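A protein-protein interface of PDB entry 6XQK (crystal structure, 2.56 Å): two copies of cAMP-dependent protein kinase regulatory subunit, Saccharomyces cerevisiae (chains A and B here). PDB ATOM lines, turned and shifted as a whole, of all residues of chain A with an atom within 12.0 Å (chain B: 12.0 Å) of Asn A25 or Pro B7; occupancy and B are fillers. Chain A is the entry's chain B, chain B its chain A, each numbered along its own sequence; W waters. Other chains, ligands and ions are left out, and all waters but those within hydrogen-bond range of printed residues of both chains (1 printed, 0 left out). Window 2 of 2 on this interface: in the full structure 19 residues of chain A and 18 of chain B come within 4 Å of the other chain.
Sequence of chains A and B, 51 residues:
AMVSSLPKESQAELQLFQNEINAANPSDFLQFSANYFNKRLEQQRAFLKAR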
ATOM      1  N   LEU A  16     -11.621  -5.686  13.526  1.00  0.00           N
ATOM      2  CA  LEU A  16     -12.036  -4.788  14.601  1.00  0.00           C
ATOM      3  C   LEU A  16     -13.485  -4.329  14.390  1.00  0.00           C
ATOM      4  O   LEU A  16     -14.260  -4.240  15.350  1.00  0.00           O
ATOM      5  CB  LEU A  16     -11.110  -3.555  14.645  1.00  0.00           C
ATOM      6  CG  LEU A  16      -9.790  -3.679  15.404  1.00  0.00           C
ATOM      7  CD1 LEU A  16      -9.073  -2.349  15.438  1.00  0.00           C
ATOM      8  CD2 LEU A  16     -10.007  -4.181  16.824  1.00  0.00           C
ATOM      9  N   PHE A  17     -13.831  -4.013  13.128  1.00  0.00           N
ATOM     10  CA  PHE A  17     -15.165  -3.581  12.741  1.00  0.00           C
ATOM     11  C   PHE A  17     -16.167  -4.711  12.945  1.00  0.00           C
ATOM     12  O   PHE A  17     -17.169  -4.501  13.621  1.00  0.00           O
ATOM     13  CB  PHE A  17     -15.170  -3.071  11.297  1.00  0.00           C
ATOM     14  CG  PHE A  17     -16.546  -2.784  10.752  1.00  0.00           C
ATOM     15  CD1 PHE A  17     -17.360  -1.822  11.338  1.00  0.00           C
ATOM     16  CD2 PHE A  17     -17.023  -3.461   9.643  1.00  0.00           C
ATOM     17  CE1 PHE A  17     -18.618  -1.547  10.823  1.00  0.00           C
ATOM     18  CE2 PHE A  17     -18.290  -3.193   9.141  1.00  0.00           C
ATOM     19  CZ  PHE A  17     -19.074  -2.236   9.726  1.00  0.00           C
ATOM     20  N   GLN A  18     -15.867  -5.919  12.442  1.00  0.00           N
ATOM     21  CA  GLN A  18     -16.741  -7.077  12.603  1.00  0.00           C
ATOM     22  C   GLN A  18     -16.964  -7.405  14.074  1.00  0.00           C
ATOM     23  O   GLN A  18     -18.073  -7.796  14.434  1.00  0.00           O
ATOM     24  CB  GLN A  18     -16.175  -8.301  11.884  1.00  0.00           C
ATOM     25  CG  GLN A  18     -16.282  -8.216  10.381  1.00  0.00           C
ATOM     26  CD  GLN A  18     -15.552  -9.345   9.681  1.00  0.00           C
ATOM     27  OE1 GLN A  18     -14.655  -9.998  10.227  1.00  0.00           O
ATOM     28  NE2 GLN A  18     -15.915  -9.578   8.435  1.00  0.00           N
ATOM     29  N   ASN A  19     -15.934  -7.225  14.922  1.00  0.00           N
ATOM     30  CA  ASN A  19     -16.047  -7.453  16.364  1.00  0.00           C
ATOM     31  C   ASN A  19     -17.009  -6.460  17.001  1.00  0.00           C
ATOM     32  O   ASN A  19     -17.805  -6.846  17.844  1.00  0.00           O
ATOM     33  CB  ASN A  19     -14.677  -7.358  17.043  1.00  0.00           C
ATOM     34  CG  ASN A  19     -13.778  -8.548  16.767  1.00  0.00           C
ATOM     35  OD1 ASN A  19     -14.193  -9.545  16.148  1.00  0.00           O
ATOM     36  ND2 ASN A  19     -12.515  -8.464  17.193  1.00  0.00           N
ATOM     37  N   GLU A  20     -16.946  -5.187  16.585  1.00  0.00           N
ATOM     38  CA  GLU A  20     -17.825  -4.121  17.055  1.00  0.00           C
ATOM     39  C   GLU A  20     -19.283  -4.359  16.663  1.00  0.00           C
ATOM     40  O   GLU A  20     -20.167  -4.136  17.483  1.00  0.00           O
ATOM     41  CB  GLU A  20     -17.350  -2.761  16.505  1.00  0.00           C
ATOM     42  CG  GLU A  20     -16.233  -2.150  17.312  1.00  0.00           C
ATOM     43  CD  GLU A  20     -16.633  -1.888  18.742  1.00  0.00           C
ATOM     44  OE1 GLU A  20     -17.695  -1.259  18.951  1.00  0.00           O
ATOM     45  OE2 GLU A  20     -15.905  -2.336  19.656  1.00  0.00           O
ATOM     46  N   ILE A  21     -19.524  -4.814  15.424  1.00  0.00           N
ATOM     47  CA  ILE A  21     -20.852  -5.130  14.918  1.00  0.00           C
ATOM     48  C   ILE A  21     -21.442  -6.293  15.711  1.00  0.00           C
ATOM     49  O   ILE A  21     -22.608  -6.229  16.086  1.00  0.00           O
ATOM     50  CB  ILE A  21     -20.804  -5.499  13.413  1.00  0.00           C
ATOM     51  CG1 ILE A  21     -20.382  -4.321  12.550  1.00  0.00           C
ATOM     52  CG2 ILE A  21     -22.140  -6.084  12.924  1.00  0.00           C
ATOM     53  CD1 ILE A  21     -21.290  -3.136  12.671  1.00  0.00           C
ATOM     54  N   ASN A  22     -20.650  -7.353  15.957  1.00  0.00           N
ATOM     55  CA  ASN A  22     -21.139  -8.497  16.710  1.00  0.00           C
ATOM     56  C   ASN A  22     -21.380  -8.179  18.177  1.00  0.00           C
ATOM     57  O   ASN A  22     -22.280  -8.768  18.783  1.00  0.00           O
ATOM     58  CB  ASN A  22     -20.190  -9.674  16.584  1.00  0.00           C
ATOM     59  CG  ASN A  22     -20.142 -10.245  15.204  1.00  0.00           C
ATOM     60  OD1 ASN A  22     -21.142 -10.222  14.454  1.00  0.00           O
ATOM     61  ND2 ASN A  22     -18.968 -10.768  14.838  1.00  0.00           N
ATOM     62  N   ALA A  23     -20.576  -7.259  18.758  1.00  0.00           N
ATOM     63  CA  ALA A  23     -20.736  -6.891  20.150  1.00  0.00           C
ATOM     64  C   ALA A  23     -21.940  -5.979  20.361  1.00  0.00           C
ATOM     65  O   ALA A  23     -22.626  -6.121  21.374  1.00  0.00           O
ATOM     66  CB  ALA A  23     -19.479  -6.219  20.664  1.00  0.00           C
ATOM     67  N   ALA A  24     -22.195  -5.037  19.424  1.00  0.00           N
ATOM     68  CA  ALA A  24     -23.264  -4.074  19.595  1.00  0.00           C
ATOM     69  C   ALA A  24     -24.586  -4.506  18.988  1.00  0.00           C
ATOM     70  O   ALA A  24     -25.649  -4.135  19.500  1.00  0.00           O
ATOM     71  CB  ALA A  24     -22.841  -2.718  19.034  1.00  0.00           C
ATOM     72  N   ASN A  25     -24.539  -5.259  17.872  1.00  0.00           N
ATOM     73  CA  ASN A  25     -25.697  -5.693  17.048  1.00  0.00           C
ATOM     74  C   ASN A  25     -26.657  -4.511  16.827  1.00  0.00           C
ATOM     75  O   ASN A  25     -27.770  -4.480  17.371  1.00  0.00           O
ATOM     76  CB  ASN A  25     -26.411  -6.892  17.647  1.00  0.00           C
ATOM     77  CG  ASN A  25     -27.371  -7.565  16.706  1.00  0.00           C
ATOM     78  OD1 ASN A  25     -27.524  -7.185  15.541  1.00  0.00           O
ATOM     79  ND2 ASN A  25     -28.028  -8.603  17.199  1.00  0.00           N
ATOM     80  N   PRO A  26     -26.137  -3.445  16.170  1.00  0.00           N
ATOM     81  CA  PRO A  26     -26.916  -2.213  16.050  1.00  0.00           C
ATOM     82  C   PRO A  26     -28.265  -2.345  15.383  1.00  0.00           C
ATOM     83  O   PRO A  26     -28.479  -3.152  14.478  1.00  0.00           O
ATOM     84  CB  PRO A  26     -26.000  -1.292  15.253  1.00  0.00           C
ATOM     85  CG  PRO A  26     -25.067  -2.221  14.537  1.00  0.00           C
ATOM     86  CD  PRO A  26     -24.825  -3.311  15.502  1.00  0.00           C
ATOM     87  N   SER A  27     -29.187  -1.520  15.887  1.00  0.00           N
ATOM     88  CA  SER A  27     -30.547  -1.323  15.393  1.00  0.00           C
ATOM     89  C   SER A  27     -30.512  -0.617  14.037  1.00  0.00           C
ATOM     90  O   SER A  27     -31.376  -0.832  13.194  1.00  0.00           O
ATOM     91  CB  SER A  27     -31.331  -0.472  16.390  1.00  0.00           C
ATOM     92  OG  SER A  27     -31.404  -1.085  17.669  1.00  0.00           O
ATOM     93  N   ASP A  28     -29.496   0.213  13.820  1.00  0.00           N
ATOM     94  CA  ASP A  28     -29.260   0.958  12.587  1.00  0.00           C
ATOM     95  C   ASP A  28     -27.821   0.616  12.157  1.00  0.00           C
ATOM     96  O   ASP A  28     -26.877   1.294  12.573  1.00  0.00           O
ATOM     97  CB  ASP A  28     -29.422   2.463  12.861  1.00  0.00           C
ATOM     98  CG  ASP A  28     -29.513   3.296  11.619  1.00  0.00           C
ATOM     99  OD1 ASP A  28     -28.924   2.893  10.599  1.00  0.00           O
ATOM    100  OD2 ASP A  28     -30.174   4.372  11.667  1.00  0.00           O
ATOM    101  N   PHE A  29     -27.662  -0.463  11.373  1.00  0.00           N
ATOM    102  CA  PHE A  29     -26.355  -0.911  10.924  1.00  0.00           C
ATOM    103  C   PHE A  29     -25.568   0.192  10.193  1.00  0.00           C
ATOM    104  O   PHE A  29     -24.406   0.412  10.516  1.00  0.00           O
ATOM    105  CB  PHE A  29     -26.482  -2.185  10.048  1.00  0.00           C
ATOM    106  CG  PHE A  29     -25.158  -2.758   9.570  1.00  0.00           C
ATOM    107  CD1 PHE A  29     -24.560  -2.293   8.407  1.00  0.00           C
ATOM    108  CD2 PHE A  29     -24.491  -3.726  10.310  1.00  0.00           C
ATOM    109  CE1 PHE A  29     -23.315  -2.772   8.008  1.00  0.00           C
ATOM    110  CE2 PHE A  29     -23.263  -4.230   9.884  1.00  0.00           C
ATOM    111  CZ  PHE A  29     -22.679  -3.744   8.743  1.00  0.00           C
ATOM    112  N   LEU A  30     -26.191   0.865   9.205  1.00  0.00           N
ATOM    113  CA  LEU A  30     -25.516   1.894   8.431  1.00  0.00           C
ATOM    114  C   LEU A  30     -25.030   3.056   9.270  1.00  0.00           C
ATOM    115  O   LEU A  30     -23.896   3.522   9.054  1.00  0.00           O
ATOM    116  CB  LEU A  30     -26.401   2.406   7.268  1.00  0.00           C
ATOM    117  CG  LEU A  30     -26.583   1.483   6.099  1.00  0.00           C
ATOM    118  CD1 LEU A  30     -27.399   2.141   5.054  1.00  0.00           C
ATOM    119  CD2 LEU A  30     -25.243   1.061   5.503  1.00  0.00           C
ATOM    120  N   GLN A  31     -25.893   3.553  10.210  1.00  0.00           N
ATOM    121  CA  GLN A  31     -25.530   4.691  11.047  1.00  0.00           C
ATOM    122  C   GLN A  31     -24.418   4.324  11.992  1.00  0.00           C
ATOM    123  O   GLN A  31     -23.495   5.113  12.166  1.00  0.00           O
ATOM    124  CB  GLN A  31     -26.736   5.238  11.783  1.00  0.00           C
ATOM    125  CG  GLN A  31     -26.466   6.565  12.476  1.00  0.00           C
ATOM    126  CD  GLN A  31     -26.171   7.690  11.512  1.00  0.00           C
ATOM    127  OE1 GLN A  31     -27.054   8.176  10.818  1.00  0.00           O
ATOM    128  NE2 GLN A  31     -24.927   8.137  11.467  1.00  0.00           N
ATOM    129  N   PHE A  32     -24.468   3.112  12.576  1.00  0.00           N
ATOM    130  CA  PHE A  32     -23.437   2.636  13.500  1.00  0.00           C
ATOM    131  C   PHE A  32     -22.117   2.506  12.772  1.00  0.00           C
ATOM    132  O   PHE A  32     -21.082   2.894  13.325  1.00  0.00           O
ATOM    133  CB  PHE A  32     -23.824   1.271  14.073  1.00  0.00           C
ATOM    134  CG  PHE A  32     -22.798   0.650  14.995  1.00  0.00           C
ATOM    135  CD1 PHE A  32     -21.789  -0.166  14.492  1.00  0.00           C
ATOM    136  CD2 PHE A  32     -22.863   0.850  16.366  1.00  0.00           C
ATOM    137  CE1 PHE A  32     -20.821  -0.712  15.339  1.00  0.00           C
ATOM    138  CE2 PHE A  32     -21.918   0.268  17.214  1.00  0.00           C
ATOM    139  CZ  PHE A  32     -20.900  -0.504  16.694  1.00  0.00           C
ATOM    140  N   SER A  33     -22.141   1.922  11.548  1.00  0.00           N
ATOM    141  CA  SER A  33     -20.937   1.705  10.755  1.00  0.00           C
ATOM    142  C   SER A  33     -20.310   3.009  10.290  1.00  0.00           C
ATOM    143  O   SER A  33     -19.097   3.153  10.365  1.00  0.00           O
ATOM    144  CB  SER A  33     -21.233   0.793   9.576  1.00  0.00           C
ATOM    145  OG  SER A  33     -21.810  -0.419  10.028  1.00  0.00           O
ATOM    146  N   TYR A  36     -18.748   4.608  13.362  1.00  0.00           N
ATOM    147  CA  TYR A  36     -17.537   3.853  13.702  1.00  0.00           C
ATOM    148  C   TYR A  36     -16.332   4.284  12.840  1.00  0.00           C
ATOM    149  O   TYR A  36     -15.265   4.587  13.381  1.00  0.00           O
ATOM    150  CB  TYR A  36     -17.793   2.332  13.580  1.00  0.00           C
ATOM    151  CG  TYR A  36     -16.544   1.508  13.800  1.00  0.00           C
ATOM    152  CD1 TYR A  36     -16.130   1.167  15.076  1.00  0.00           C
ATOM    153  CD2 TYR A  36     -15.742   1.111  12.727  1.00  0.00           C
ATOM    154  CE1 TYR A  36     -14.956   0.453  15.286  1.00  0.00           C
ATOM    155  CE2 TYR A  36     -14.564   0.405  12.926  1.00  0.00           C
ATOM    156  CZ  TYR A  36     -14.176   0.073  14.205  1.00  0.00           C
ATOM    157  OH  TYR A  36     -13.007  -0.635  14.383  1.00  0.00           O
ATOM    158  N   SER B   5     -24.303 -14.072  14.581  1.00  0.00           N
ATOM    159  CA  SER B   5     -25.734 -14.411  14.664  1.00  0.00           C
ATOM    160  C   SER B   5     -26.697 -13.250  14.220  1.00  0.00           C
ATOM    161  O   SER B   5     -27.924 -13.381  14.363  1.00  0.00           O
ATOM    162  CB  SER B   5     -26.081 -14.880  16.073  1.00  0.00           C
ATOM    163  N   LEU B   6     -26.115 -12.138  13.692  1.00  0.00           N
ATOM    164  CA  LEU B   6     -26.735 -10.892  13.209  1.00  0.00           C
ATOM    165  C   LEU B   6     -28.049 -11.046  12.443  1.00  0.00           C
ATOM    166  O   LEU B   6     -28.223 -12.000  11.690  1.00  0.00           O
ATOM    167  CB  LEU B   6     -25.743 -10.171  12.244  1.00  0.00           C
ATOM    168  CG  LEU B   6     -24.400  -9.785  12.793  1.00  0.00           C
ATOM    169  CD1 LEU B   6     -23.511  -9.268  11.699  1.00  0.00           C
ATOM    170  CD2 LEU B   6     -24.547  -8.755  13.915  1.00  0.00           C
ATOM    171  N   PRO B   7     -28.921 -10.028  12.489  1.00  0.00           N
ATOM    172  CA  PRO B   7     -30.114 -10.036  11.635  1.00  0.00           C
ATOM    173  C   PRO B   7     -29.752 -10.123  10.138  1.00  0.00           C
ATOM    174  O   PRO B   7     -28.623  -9.818   9.715  1.00  0.00           O
ATOM    175  CB  PRO B   7     -30.770  -8.677  11.935  1.00  0.00           C
ATOM    176  CG  PRO B   7     -30.191  -8.222  13.185  1.00  0.00           C
ATOM    177  CD  PRO B   7     -28.830  -8.791  13.278  1.00  0.00           C
ATOM    178  N   LYS B   8     -30.728 -10.530   9.334  1.00  0.00           N
ATOM    179  CA  LYS B   8     -30.549 -10.683   7.901  1.00  0.00           C
ATOM    180  C   LYS B   8     -30.147  -9.382   7.212  1.00  0.00           C
ATOM    181  O   LYS B   8     -29.246  -9.433   6.393  1.00  0.00           O
ATOM    182  CB  LYS B   8     -31.811 -11.280   7.276  1.00  0.00           C
ATOM    183  N   GLU B   9     -30.761  -8.227   7.552  1.00  0.00           N
ATOM    184  CA  GLU B   9     -30.401  -6.948   6.925  1.00  0.00           C
ATOM    185  C   GLU B   9     -28.962  -6.557   7.235  1.00  0.00           C
ATOM    186  O   GLU B   9     -28.262  -6.061   6.349  1.00  0.00           O
ATOM    187  CB  GLU B   9     -31.352  -5.824   7.355  1.00  0.00           C
ATOM    188  CG  GLU B   9     -31.105  -4.502   6.624  1.00  0.00           C
ATOM    189  CD  GLU B   9     -32.019  -3.354   7.012  1.00  0.00           C
ATOM    190  OE1 GLU B   9     -33.140  -3.627   7.498  1.00  0.00           O
ATOM    191  OE2 GLU B   9     -31.620  -2.180   6.825  1.00  0.00           O
ATOM    192  N   SER B  10     -28.513  -6.813   8.474  1.00  0.00           N
ATOM    193  CA  SER B  10     -27.144  -6.542   8.912  1.00  0.00           C
ATOM    194  C   SER B  10     -26.127  -7.428   8.172  1.00  0.00           C
ATOM    195  O   SER B  10     -25.085  -6.940   7.738  1.00  0.00           O
ATOM    196  CB  SER B  10     -27.027  -6.738  10.418  1.00  0.00           C
ATOM    197  OG  SER B  10     -27.890  -5.837  11.086  1.00  0.00           O
ATOM    198  N   GLN B  11     -26.453  -8.724   8.008  1.00  0.00           N
ATOM    199  CA  GLN B  11     -25.591  -9.631   7.270  1.00  0.00           C
ATOM    200  C   GLN B  11     -25.493  -9.228   5.805  1.00  0.00           C
ATOM    201  O   GLN B  11     -24.423  -9.335   5.219  1.00  0.00           O
ATOM    202  CB  GLN B  11     -26.079 -11.070   7.402  1.00  0.00           C
ATOM    203  CG  GLN B  11     -26.010 -11.525   8.845  1.00  0.00           C
ATOM    204  CD  GLN B  11     -25.583 -12.942   9.066  1.00  0.00           C
ATOM    205  OE1 GLN B  11     -24.763 -13.229   9.962  1.00  0.00           O
ATOM    206  NE2 GLN B  11     -26.123 -13.857   8.273  1.00  0.00           N
ATOM    207  N   ALA B  12     -26.598  -8.732   5.216  1.00  0.00           N
ATOM    208  CA  ALA B  12     -26.629  -8.282   3.818  1.00  0.00           C
ATOM    209  C   ALA B  12     -25.755  -7.054   3.629  1.00  0.00           C
ATOM    210  O   ALA B  12     -24.939  -7.037   2.705  1.00  0.00           O
ATOM    211  CB  ALA B  12     -28.056  -7.994   3.393  1.00  0.00           C
ATOM    212  N   GLU B  13     -25.871  -6.048   4.531  1.00  0.00           N
ATOM    213  CA  GLU B  13     -25.046  -4.845   4.452  1.00  0.00           C
ATOM    214  C   GLU B  13     -23.559  -5.132   4.707  1.00  0.00           C
ATOM    215  O   GLU B  13     -22.686  -4.495   4.109  1.00  0.00           O
ATOM    216  CB  GLU B  13     -25.539  -3.774   5.430  1.00  0.00           C
ATOM    217  CG  GLU B  13     -26.881  -3.196   5.077  1.00  0.00           C
ATOM    218  CD  GLU B  13     -26.890  -2.155   3.970  1.00  0.00           C
ATOM    219  OE1 GLU B  13     -25.837  -1.873   3.347  1.00  0.00           O
ATOM    220  OE2 GLU B  13     -27.988  -1.607   3.734  1.00  0.00           O
ATOM    221  N   LEU B  14     -23.278  -6.091   5.584  1.00  0.00           N
ATOM    222  CA  LEU B  14     -21.908  -6.489   5.871  1.00  0.00           C
ATOM    223  C   LEU B  14     -21.321  -7.241   4.681  1.00  0.00           C
ATOM    224  O   LEU B  14     -20.172  -7.013   4.331  1.00  0.00           O
ATOM    225  CB  LEU B  14     -21.853  -7.339   7.142  1.00  0.00           C
ATOM    226  CG  LEU B  14     -20.474  -7.734   7.603  1.00  0.00           C
ATOM    227  CD1 LEU B  14     -19.635  -6.524   7.941  1.00  0.00           C
ATOM    228  CD2 LEU B  14     -20.554  -8.653   8.800  1.00  0.00           C
ATOM    229  N   GLN B  15     -22.117  -8.092   4.013  1.00  0.00           N
ATOM    230  CA  GLN B  15     -21.667  -8.840   2.838  1.00  0.00           C
ATOM    231  C   GLN B  15     -21.391  -7.887   1.661  1.00  0.00           C
ATOM    232  O   GLN B  15     -20.428  -8.072   0.927  1.00  0.00           O
ATOM    233  CB  GLN B  15     -22.679  -9.931   2.463  1.00  0.00           C
ATOM    234  CG  GLN B  15     -22.125 -11.039   1.567  1.00  0.00           C
ATOM    235  CD  GLN B  15     -20.887 -11.769   2.111  1.00  0.00           C
ATOM    236  OE1 GLN B  15     -20.936 -12.467   3.140  1.00  0.00           O
ATOM    237  NE2 GLN B  15     -19.745 -11.650   1.420  1.00  0.00           N
ATOM    238  N   LEU B  16     -22.213  -6.852   1.501  1.00  0.00           N
ATOM    239  CA  LEU B  16     -22.017  -5.856   0.448  1.00  0.00           C
ATOM    240  C   LEU B  16     -20.712  -5.072   0.687  1.00  0.00           C
ATOM    241  O   LEU B  16     -19.964  -4.769  -0.256  1.00  0.00           O
ATOM    242  CB  LEU B  16     -23.197  -4.877   0.439  1.00  0.00           C
ATOM    243  CG  LEU B  16     -24.464  -5.257  -0.315  1.00  0.00           C
ATOM    244  CD1 LEU B  16     -25.400  -4.066  -0.371  1.00  0.00           C
ATOM    245  CD2 LEU B  16     -24.157  -5.719  -1.729  1.00  0.00           C
ATOM    246  N   GLN B  18     -18.025  -6.121   2.620  1.00  0.00           N
ATOM    247  CA  GLN B  18     -16.907  -7.042   2.447  1.00  0.00           C
ATOM    248  C   GLN B  18     -16.596  -7.274   0.964  1.00  0.00           C
ATOM    249  O   GLN B  18     -15.425  -7.403   0.604  1.00  0.00           O
ATOM    250  CB  GLN B  18     -17.197  -8.375   3.139  1.00  0.00           C
ATOM    251  CG  GLN B  18     -17.068  -8.307   4.638  1.00  0.00           C
ATOM    252  CD  GLN B  18     -17.536  -9.580   5.314  1.00  0.00           C
ATOM    253  OE1 GLN B  18     -18.032  -9.552   6.439  1.00  0.00           O
ATOM    254  NE2 GLN B  18     -17.383 -10.739   4.671  1.00  0.00           N
HETATM  255  O   HOH W   1     -27.382  -5.384  13.563  1.00  0.00           O
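OE1 of Gln B18 lies within hydrogen-bond range of NE2 of Gln A18.
The backbone carbonyl oxygen (O) of Phe A29 lies within hydrogen-bond range of the side-chain hydroxyl (OG) of Ser A33 (2.8 Å). The backbone carbonyl oxygen (O) of Gln A18 is in hydrogen-bond range of the side-chain amide nitrogen (ND2) of Asn A22 (3.1 Å).
Among the printed residues, merely in contact across the chains: Asn A25 with Pro B7 (3.1 Å), Phe A29 with Glu B13 (3.5 Å), Ile A21 with Leu B6 (3.7 Å), Asn A22 with Leu B6 (3.7 Å), Leu A30 with Glu B13 (3.7 Å), Asn A25 with Leu B6 (3.7 Å), Phe A17 with Leu B14 (3.8 Å), Phe A29 with Ser B10 (3.9 Å) and Phe A29 with Leu B14 (3.98 Å).
Of the printed residues of chain B, Phe A17 touches Leu B14. Of the printed residues of chain B, Gln A18 touches Gln B18. Ile A21 touches just one residue of chain B: Leu B6. No residue of chain B comes within 4 Å of Ala A24. Asn A25 touches just these residues of chain B: Leu B6 (3.7 Å) and Pro B7 (3.1 Å). No residue of chain B comes within 4 Å of Pro A26. No residue of chain B comes within 4 Å of Ser A27. Printed residues of chain B within 4 Å of Leu A30: Glu B13. Gln A31 touches none of the printed residues of chain B. Leu B6 touches just these residues of chain A: Ile A21 (3.7 Å), Asn A22 (3.7 Å) and Asn A25 (3.7 Å). Of chain A, only Asn A25 comes within 4 Å of Pro B7. No residue of chain A comes within 4 Å of Gln B11. The nearest residue of chain B that does not touch Asn A25 is Ser B10 (4.7 Å). The nearest residue of chain A that does not touch Pro B7 is Pro A26 (5.5 Å).
Hydrophobic or aromatic side chains of chain B that line the printed part of chain A: Leu B6, Pro B7 and Leu B14. Along chain B the printed residues that touch a printed residue of chain A span positions 6 to 18. Of the 19 printed residues of chain A, 7 touch a printed residue of chain B. Printed residues of chain A that touch a printed residue of chain B: Phe A17, Gln A18, Ile A21, Asn A22, Asn A25, Phe A29 and Leu A30. Hydrophobic or aromatic side chains of chain A that line the printed part of chain B: Phe A17, Ile A21, Phe A29 and Leu A30.
Gln A18 touches its own counterpart, Gln B18. 2 positions are printed for both chains. Of the 10 pairs that touch across the chains among the printed residues, 1 has its exchanged pair printed and touching as well.
Water W1 lies within hydrogen-bond range of OG of Ser B10 (2.6 Å), O of Pro A26 (2.6 Å) and OD1 of Asn A25 (2.7 Å).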
